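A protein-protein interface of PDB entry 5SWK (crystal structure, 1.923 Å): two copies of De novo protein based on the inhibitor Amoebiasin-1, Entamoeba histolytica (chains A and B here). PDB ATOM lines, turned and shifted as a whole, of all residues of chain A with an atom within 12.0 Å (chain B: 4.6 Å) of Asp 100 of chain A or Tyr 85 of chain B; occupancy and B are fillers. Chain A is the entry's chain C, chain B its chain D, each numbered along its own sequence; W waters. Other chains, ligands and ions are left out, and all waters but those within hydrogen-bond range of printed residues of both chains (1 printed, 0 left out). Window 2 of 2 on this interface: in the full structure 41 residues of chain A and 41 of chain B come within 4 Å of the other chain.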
ATOM      1  N   ALA A  91      10.840  30.234   8.350  1.00  0.00           N
ATOM      2  CA  ALA A  91      11.653  30.014   9.549  1.00  0.00           C
ATOM      3  C   ALA A  91      11.140  28.837  10.356  1.00  0.00           C
ATOM      4  O   ALA A  91      11.928  28.046  10.885  1.00  0.00           O
ATOM      5  CB  ALA A  91      11.688  31.282  10.429  1.00  0.00           C
ATOM      6  N   GLU A  92       9.818  28.710  10.447  1.00  0.00           N
ATOM      7  CA  GLU A  92       9.227  27.614  11.207  1.00  0.00           C
ATOM      8  C   GLU A  92       9.497  26.275  10.530  1.00  0.00           C
ATOM      9  O   GLU A  92       9.854  25.299  11.192  1.00  0.00           O
ATOM     10  CB  GLU A  92       7.725  27.841  11.405  1.00  0.00           C
ATOM     11  CG  GLU A  92       7.432  28.981  12.393  1.00  0.00           C
ATOM     12  CD  GLU A  92       5.955  29.346  12.494  1.00  0.00           C
ATOM     13  OE1 GLU A  92       5.282  29.455  11.449  1.00  0.00           O
ATOM     14  OE2 GLU A  92       5.473  29.544  13.630  1.00  0.00           O
ATOM     15  N   TYR A  93       9.343  26.229   9.209  1.00  0.00           N
ATOM     16  CA  TYR A  93       9.695  25.023   8.460  1.00  0.00           C
ATOM     17  C   TYR A  93      11.174  24.664   8.606  1.00  0.00           C
ATOM     18  O   TYR A  93      11.532  23.518   8.885  1.00  0.00           O
ATOM     19  CB  TYR A  93       9.361  25.208   6.982  1.00  0.00           C
ATOM     20  CG  TYR A  93       7.892  25.050   6.663  1.00  0.00           C
ATOM     21  CD1 TYR A  93       7.238  23.850   6.907  1.00  0.00           C
ATOM     22  CD2 TYR A  93       7.168  26.087   6.100  1.00  0.00           C
ATOM     23  CE1 TYR A  93       5.894  23.691   6.609  1.00  0.00           C
ATOM     24  CE2 TYR A  93       5.816  25.930   5.779  1.00  0.00           C
ATOM     25  CZ  TYR A  93       5.190  24.731   6.045  1.00  0.00           C
ATOM     26  OH  TYR A  93       3.853  24.560   5.739  1.00  0.00           O
ATOM     27  N   TRP A  94      12.031  25.655   8.406  1.00  0.00           N
ATOM     28  CA  TRP A  94      13.467  25.417   8.390  1.00  0.00           C
ATOM     29  C   TRP A  94      13.986  24.936   9.743  1.00  0.00           C
ATOM     30  O   TRP A  94      14.868  24.079   9.812  1.00  0.00           O
ATOM     31  CB  TRP A  94      14.209  26.680   7.966  1.00  0.00           C
ATOM     32  CG  TRP A  94      15.658  26.426   7.685  1.00  0.00           C
ATOM     33  CD1 TRP A  94      16.719  26.699   8.505  1.00  0.00           C
ATOM     34  CD2 TRP A  94      16.203  25.831   6.502  1.00  0.00           C
ATOM     35  NE1 TRP A  94      17.895  26.314   7.898  1.00  0.00           N
ATOM     36  CE2 TRP A  94      17.602  25.777   6.668  1.00  0.00           C
ATOM     37  CE3 TRP A  94      15.641  25.341   5.314  1.00  0.00           C
ATOM     38  CZ2 TRP A  94      18.448  25.250   5.694  1.00  0.00           C
ATOM     39  CZ3 TRP A  94      16.486  24.819   4.342  1.00  0.00           C
ATOM     40  CH2 TRP A  94      17.875  24.776   4.542  1.00  0.00           C
ATOM     41  N   ASN A  95      13.426  25.489  10.811  1.00  0.00           N
ATOM     42  CA  ASN A  95      13.801  25.119  12.169  1.00  0.00           C
ATOM     43  C   ASN A  95      13.652  23.611  12.421  1.00  0.00           C
ATOM     44  O   ASN A  95      14.407  23.021  13.190  1.00  0.00           O
ATOM     45  CB  ASN A  95      12.955  25.923  13.163  1.00  0.00           C
ATOM     46  CG  ASN A  95      13.665  26.172  14.477  1.00  0.00           C
ATOM     47  OD1 ASN A  95      14.487  25.369  14.914  1.00  0.00           O
ATOM     48  ND2 ASN A  95      13.343  27.294  15.122  1.00  0.00           N
ATOM     49  N   LEU A  96      12.691  22.981  11.749  1.00  0.00           N
ATOM     50  CA  LEU A  96      12.420  21.563  11.982  1.00  0.00           C
ATOM     51  C   LEU A  96      13.495  20.621  11.416  1.00  0.00           C
ATOM     52  O   LEU A  96      13.500  19.429  11.726  1.00  0.00           O
ATOM     53  CB  LEU A  96      11.051  21.190  11.410  1.00  0.00           C
ATOM     54  CG  LEU A  96       9.849  21.873  12.077  1.00  0.00           C
ATOM     55  CD1 LEU A  96       8.564  21.526  11.351  1.00  0.00           C
ATOM     56  CD2 LEU A  96       9.751  21.499  13.561  1.00  0.00           C
ATOM     57  N   LEU A  97      14.406  21.153  10.601  1.00  0.00           N
ATOM     58  CA  LEU A  97      15.528  20.369  10.077  1.00  0.00           C
ATOM     59  C   LEU A  97      16.560  20.119  11.166  1.00  0.00           C
ATOM     60  O   LEU A  97      17.438  19.272  11.022  1.00  0.00           O
ATOM     61  CB  LEU A  97      16.188  21.083   8.898  1.00  0.00           C
ATOM     62  CG  LEU A  97      15.380  21.180   7.606  1.00  0.00           C
ATOM     63  CD1 LEU A  97      16.065  22.137   6.653  1.00  0.00           C
ATOM     64  CD2 LEU A  97      15.248  19.809   6.956  1.00  0.00           C
ATOM     65  N   SER A  98      16.464  20.897  12.240  1.00  0.00           N
ATOM     66  CA  SER A  98      17.320  20.733  13.408  1.00  0.00           C
ATOM     67  C   SER A  98      16.431  20.478  14.608  1.00  0.00           C
ATOM     68  O   SER A  98      16.183  21.382  15.399  1.00  0.00           O
ATOM     69  CB  SER A  98      18.179  21.969  13.644  1.00  0.00           C
ATOM     70  OG  SER A  98      18.845  22.362  12.462  1.00  0.00           O
ATOM     71  N   PRO A  99      15.931  19.243  14.729  1.00  0.00           N
ATOM     72  CA  PRO A  99      14.912  18.939  15.732  1.00  0.00           C
ATOM     73  C   PRO A  99      15.436  19.125  17.149  1.00  0.00           C
ATOM     74  O   PRO A  99      16.582  18.793  17.444  1.00  0.00           O
ATOM     75  CB  PRO A  99      14.569  17.469  15.452  1.00  0.00           C
ATOM     76  CG  PRO A  99      15.794  16.919  14.791  1.00  0.00           C
ATOM     77  CD  PRO A  99      16.344  18.047  13.970  1.00  0.00           C
ATOM     78  N   ASP A 100      14.594  19.687  18.005  1.00  0.00           N
ATOM     79  CA  ASP A 100      14.922  19.826  19.414  1.00  0.00           C
ATOM     80  C   ASP A 100      14.787  18.489  20.135  1.00  0.00           C
ATOM     81  O   ASP A 100      13.930  17.671  19.780  1.00  0.00           O
ATOM     82  CB  ASP A 100      14.020  20.872  20.059  1.00  0.00           C
ATOM     83  CG  ASP A 100      14.239  22.261  19.487  1.00  0.00           C
ATOM     84  OD1 ASP A 100      13.241  22.966  19.229  1.00  0.00           O
ATOM     85  OD2 ASP A 100      15.415  22.640  19.301  1.00  0.00           O
ATOM     86  N   ARG A 101      15.639  18.265  21.134  1.00  0.00           N
ATOM     87  CA  ARG A 101      15.501  17.101  22.000  1.00  0.00           C
ATOM     88  C   ARG A 101      14.114  17.119  22.630  1.00  0.00           C
ATOM     89  O   ARG A 101      13.616  18.178  23.008  1.00  0.00           O
ATOM     90  CB  ARG A 101      16.588  17.084  23.076  1.00  0.00           C
ATOM     91  N   THR A 102      13.472  15.957  22.699  1.00  0.00           N
ATOM     92  CA  THR A 102      12.139  15.864  23.277  1.00  0.00           C
ATOM     93  C   THR A 102      12.067  14.771  24.335  1.00  0.00           C
ATOM     94  O   THR A 102      12.831  13.808  24.307  1.00  0.00           O
ATOM     95  CB  THR A 102      11.058  15.568  22.212  1.00  0.00           C
ATOM     96  OG1 THR A 102      11.290  14.268  21.656  1.00  0.00           O
ATOM     97  CG2 THR A 102      11.084  16.606  21.104  1.00  0.00           C
ATOM     98  N   PHE A 103      11.137  14.929  25.269  1.00  0.00           N
ATOM     99  CA  PHE A 103      10.882  13.902  26.267  1.00  0.00           C
ATOM    100  C   PHE A 103       9.415  13.533  26.227  1.00  0.00           C
ATOM    101  O   PHE A 103       8.547  14.403  26.328  1.00  0.00           O
ATOM    102  CB  PHE A 103      11.267  14.372  27.675  1.00  0.00           C
ATOM    103  CG  PHE A 103      11.072  13.322  28.729  1.00  0.00           C
ATOM    104  CD1 PHE A 103      12.074  12.401  29.003  1.00  0.00           C
ATOM    105  CD2 PHE A 103       9.878  13.233  29.422  1.00  0.00           C
ATOM    106  CE1 PHE A 103      11.893  11.422  29.965  1.00  0.00           C
ATOM    107  CE2 PHE A 103       9.690  12.254  30.389  1.00  0.00           C
ATOM    108  CZ  PHE A 103      10.701  11.353  30.660  1.00  0.00           C
ATOM    109  N   THR A 104       9.141  12.240  26.092  1.00  0.00           N
ATOM    110  CA  THR A 104       7.776  11.774  25.932  1.00  0.00           C
ATOM    111  C   THR A 104       7.393  10.683  26.930  1.00  0.00           C
ATOM    112  O   THR A 104       8.116   9.700  27.113  1.00  0.00           O
ATOM    113  CB  THR A 104       7.545  11.230  24.514  1.00  0.00           C
ATOM    114  OG1 THR A 104       7.927  12.225  23.558  1.00  0.00           O
ATOM    115  CG2 THR A 104       6.084  10.872  24.320  1.00  0.00           C
ATOM    116  N   GLY B  29      19.294  20.288  32.436  1.00  0.00           N
ATOM    117  CA  GLY B  29      19.180  21.392  31.506  1.00  0.00           C
ATOM    118  C   GLY B  29      20.193  22.458  31.881  1.00  0.00           C
ATOM    119  O   GLY B  29      20.686  22.493  33.018  1.00  0.00           O
ATOM    120  N   ASN B  30      20.526  23.309  30.918  1.00  0.00           N
ATOM    121  CA  ASN B  30      21.425  24.426  31.165  1.00  0.00           C
ATOM    122  C   ASN B  30      20.903  25.715  30.548  1.00  0.00           C
ATOM    123  O   ASN B  30      21.277  26.068  29.427  1.00  0.00           O
ATOM    124  CB  ASN B  30      22.820  24.137  30.623  1.00  0.00           C
ATOM    125  CG  ASN B  30      23.849  25.099  31.176  1.00  0.00           C
ATOM    126  OD1 ASN B  30      23.498  26.082  31.841  1.00  0.00           O
ATOM    127  ND2 ASN B  30      25.119  24.826  30.914  1.00  0.00           N
ATOM    128  N   THR B  33      22.403  28.782  28.325  1.00  0.00           N
ATOM    129  CA  THR B  33      22.524  28.727  26.870  1.00  0.00           C
ATOM    130  C   THR B  33      21.312  29.356  26.207  1.00  0.00           C
ATOM    131  O   THR B  33      21.311  29.616  25.003  1.00  0.00           O
ATOM    132  CB  THR B  33      22.649  27.278  26.349  1.00  0.00           C
ATOM    133  OG1 THR B  33      21.463  26.551  26.692  1.00  0.00           O
ATOM    134  CG2 THR B  33      23.858  26.590  26.957  1.00  0.00           C
ATOM    135  N   TYR B  35      18.434  27.706  26.235  1.00  0.00           N
ATOM    136  CA  TYR B  35      17.500  26.574  26.135  1.00  0.00           C
ATOM    137  C   TYR B  35      16.820  26.306  27.468  1.00  0.00           C
ATOM    138  O   TYR B  35      17.390  26.571  28.526  1.00  0.00           O
ATOM    139  CB  TYR B  35      18.223  25.305  25.663  1.00  0.00           C
ATOM    140  CG  TYR B  35      18.540  25.290  24.188  1.00  0.00           C
ATOM    141  CD1 TYR B  35      19.664  25.941  23.691  1.00  0.00           C
ATOM    142  CD2 TYR B  35      17.716  24.616  23.285  1.00  0.00           C
ATOM    143  CE1 TYR B  35      19.959  25.928  22.329  1.00  0.00           C
ATOM    144  CE2 TYR B  35      18.007  24.595  21.917  1.00  0.00           C
ATOM    145  CZ  TYR B  35      19.131  25.255  21.455  1.00  0.00           C
ATOM    146  OH  TYR B  35      19.440  25.250  20.116  1.00  0.00           O
ATOM    147  N   SER B  36      15.600  25.784  27.418  1.00  0.00           N
ATOM    148  CA  SER B  36      14.924  25.308  28.613  1.00  0.00           C
ATOM    149  C   SER B  36      13.964  24.171  28.258  1.00  0.00           C
ATOM    150  O   SER B  36      13.565  24.028  27.102  1.00  0.00           O
ATOM    151  CB  SER B  36      14.165  26.447  29.298  1.00  0.00           C
ATOM    152  OG  SER B  36      13.123  26.924  28.468  1.00  0.00           O
ATOM    153  N   TRP B  37      13.603  23.363  29.250  1.00  0.00           N
ATOM    154  CA  TRP B  37      12.571  22.352  29.061  1.00  0.00           C
ATOM    155  C   TRP B  37      11.196  22.990  29.197  1.00  0.00           C
ATOM    156  O   TRP B  37      10.910  23.662  30.188  1.00  0.00           O
ATOM    157  CB  TRP B  37      12.735  21.209  30.068  1.00  0.00           C
ATOM    158  CG  TRP B  37      13.831  20.254  29.708  1.00  0.00           C
ATOM    159  CD1 TRP B  37      15.065  20.171  30.272  1.00  0.00           C
ATOM    160  CD2 TRP B  37      13.780  19.243  28.692  1.00  0.00           C
ATOM    161  NE1 TRP B  37      15.793  19.167  29.667  1.00  0.00           N
ATOM    162  CE2 TRP B  37      15.024  18.584  28.695  1.00  0.00           C
ATOM    163  CE3 TRP B  37      12.802  18.836  27.777  1.00  0.00           C
ATOM    164  CZ2 TRP B  37      15.318  17.532  27.821  1.00  0.00           C
ATOM    165  CZ3 TRP B  37      13.095  17.793  26.906  1.00  0.00           C
ATOM    166  CH2 TRP B  37      14.346  17.155  26.933  1.00  0.00           C
ATOM    167  N   LEU B  83       7.601  16.930  26.293  1.00  0.00           N
ATOM    168  CA  LEU B  83       8.434  18.057  26.676  1.00  0.00           C
ATOM    169  C   LEU B  83       9.490  18.258  25.610  1.00  0.00           C
ATOM    170  O   LEU B  83       9.978  17.296  25.019  1.00  0.00           O
ATOM    171  CB  LEU B  83       9.100  17.814  28.032  1.00  0.00           C
ATOM    172  CG  LEU B  83       8.205  17.358  29.186  1.00  0.00           C
ATOM    173  CD1 LEU B  83       9.049  17.062  30.419  1.00  0.00           C
ATOM    174  CD2 LEU B  83       7.168  18.417  29.495  1.00  0.00           C
ATOM    175  N   VAL B  84       9.851  19.510  25.367  1.00  0.00           N
ATOM    176  CA  VAL B  84      10.869  19.802  24.383  1.00  0.00           C
ATOM    177  C   VAL B  84      11.924  20.754  24.961  1.00  0.00           C
ATOM    178  O   VAL B  84      11.600  21.691  25.691  1.00  0.00           O
ATOM    179  CB  VAL B  84      10.227  20.382  23.098  1.00  0.00           C
ATOM    180  CG1 VAL B  84       9.402  21.609  23.413  1.00  0.00           C
ATOM    181  CG2 VAL B  84      11.276  20.689  22.066  1.00  0.00           C
ATOM    182  N   TYR B  85      13.188  20.472  24.665  1.00  0.00           N
ATOM    183  CA  TYR B  85      14.298  21.308  25.103  1.00  0.00           C
ATOM    184  C   TYR B  85      14.598  22.298  23.986  1.00  0.00           C
ATOM    185  O   TYR B  85      15.291  21.958  23.022  1.00  0.00           O
ATOM    186  CB  TYR B  85      15.523  20.445  25.429  1.00  0.00           C
ATOM    187  CG  TYR B  85      16.669  21.152  26.124  1.00  0.00           C
ATOM    188  CD1 TYR B  85      16.534  21.626  27.427  1.00  0.00           C
ATOM    189  CD2 TYR B  85      17.898  21.303  25.494  1.00  0.00           C
ATOM    190  CE1 TYR B  85      17.585  22.256  28.073  1.00  0.00           C
ATOM    191  CE2 TYR B  85      18.958  21.928  26.128  1.00  0.00           C
ATOM    192  CZ  TYR B  85      18.796  22.401  27.419  1.00  0.00           C
ATOM    193  OH  TYR B  85      19.854  23.016  28.051  1.00  0.00           O
ATOM    194  N   ARG B  86      14.062  23.509  24.101  1.00  0.00           N
ATOM    195  CA  ARG B  86      14.132  24.453  22.991  1.00  0.00           C
ATOM    196  C   ARG B  86      14.554  25.859  23.414  1.00  0.00           C
ATOM    197  O   ARG B  86      14.573  26.194  24.600  1.00  0.00           O
ATOM    198  CB  ARG B  86      12.782  24.524  22.270  1.00  0.00           C
ATOM    199  CG  ARG B  86      11.680  25.180  23.080  1.00  0.00           C
ATOM    200  CD  ARG B  86      10.479  25.523  22.203  1.00  0.00           C
HETATM  201  O   HOH W   1      17.268  20.422  21.890  1.00  0.00           O
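The backbone carbonyl oxygen of Arg 101 of chain A is in hydrogen-bond range of the backbone NH of Tyr 85 of chain B (2.9 Å). The backbone NH (N) of Phe 103 of chain A is in hydrogen-bond range of the backbone carbonyl oxygen (O) of Leu 83 of chain B (2.6 Å).
Water W1 lies within hydrogen-bond range of the backbone carbonyl oxygen of Tyr 85 of chain B (2.7 Å) and the backbone NH of Arg 101 of chain A (2.8 Å).
Tyr 85 of chain B touches just these residues of chain A: Asp 100 (3.4 Å) and Arg 101 (2.9 Å). No residue of chain A comes within 4 Å of Gly 29 of chain B. No residue of chain A comes within 4 Å of Asn 30 of chain B. No residue of chain A comes within 4 Å of Thr 33 of chain B. No residue of chain A comes within 4 Å of Tyr 35 of chain B. No residue of chain A comes within 4 Å of Ser 36 of chain B. Arg 86 of chain B touches just one residue of chain A: Asp 100 (3.4 Å). Printed residues of chain B within 4 Å of Phe 103 of chain A: Trp 37 (3.8 Å) and Leu 83 (2.6 Å). Printed residues of chain A within 4 Å of Leu 83 of chain B: Thr 102 and Phe 103. Of the printed residues of chain B, Thr 102 of chain A touches Leu 83. Asn 95 of chain A touches none of the printed residues of chain B. Leu 97 of chain A touches none of the printed residues of chain B. The nearest residue of chain B that does not touch Asp 100 of chain A is Tyr 35 of chain B (4.2 Å). The nearest residue of chain A that does not touch Tyr 85 of chain B is Thr 102 of chain A (4.9 Å). The nearest printed residue of chain B that does not touch Phe 103 of chain A is Val 84 of chain B (4.8 Å).
Asp 100 of chain A touches Val 84 of chain B. Tyr 85 of chain B touches Asp 100 of chain A (O to CB, 3.4 Å). Asp 100 of chain A touches Arg 86 of chain B (OD1 to CB, 3.4 Å). Arg 101 of chain A touches Trp 37 of chain B (O to CZ3, 3.95 Å). CA of Val 84 of chain B touches O of Arg 101 of chain A (3.5 Å). Thr 102 of chain A touches Leu 83 of chain B. Trp 37 of chain B touches Phe 103 of chain A.
No position is printed for both chains. Of the 9 pairs that touch across the chains among the printed residues, none has its exchanged pair printed and touching as well.
The backbone NH (N) of Asn 30 of chain B is in hydrogen-bond range of the side-chain hydroxyl (OH) of Tyr 85 of chain B, 3.0 Å away. The backbone NH (N) of Ser 36 of chain B lies within hydrogen-bond range of the backbone carbonyl oxygen (O) of Arg 86 of chain B, 3.0 Å away.
Printed residues of chain B that touch a printed residue of chain A: Trp 37, Leu 83, Val 84, Tyr 85 and Arg 86. Hydrophobic or aromatic side chains of chain B within 4 Å of the printed part of chain A: Trp 37, Leu 83, Val 84 and Tyr 85. Of the 14 printed residues of chain A, 4 touch a printed residue of chain B. Printed residues of chain A that touch a printed residue of chain B: Asp 100, Arg 101, Thr 102 and Phe 103. Hydrophobic or aromatic side chains of chain A that line the printed part of chain B: Phe 103. Along chain A the printed residues that touch a printed residue of chain B span positions 100 to 103. Among the printed residues, no Asp or Glu carboxylate lies within 4 Å of a Lys or Arg side-chain nitrogen of the other chain.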
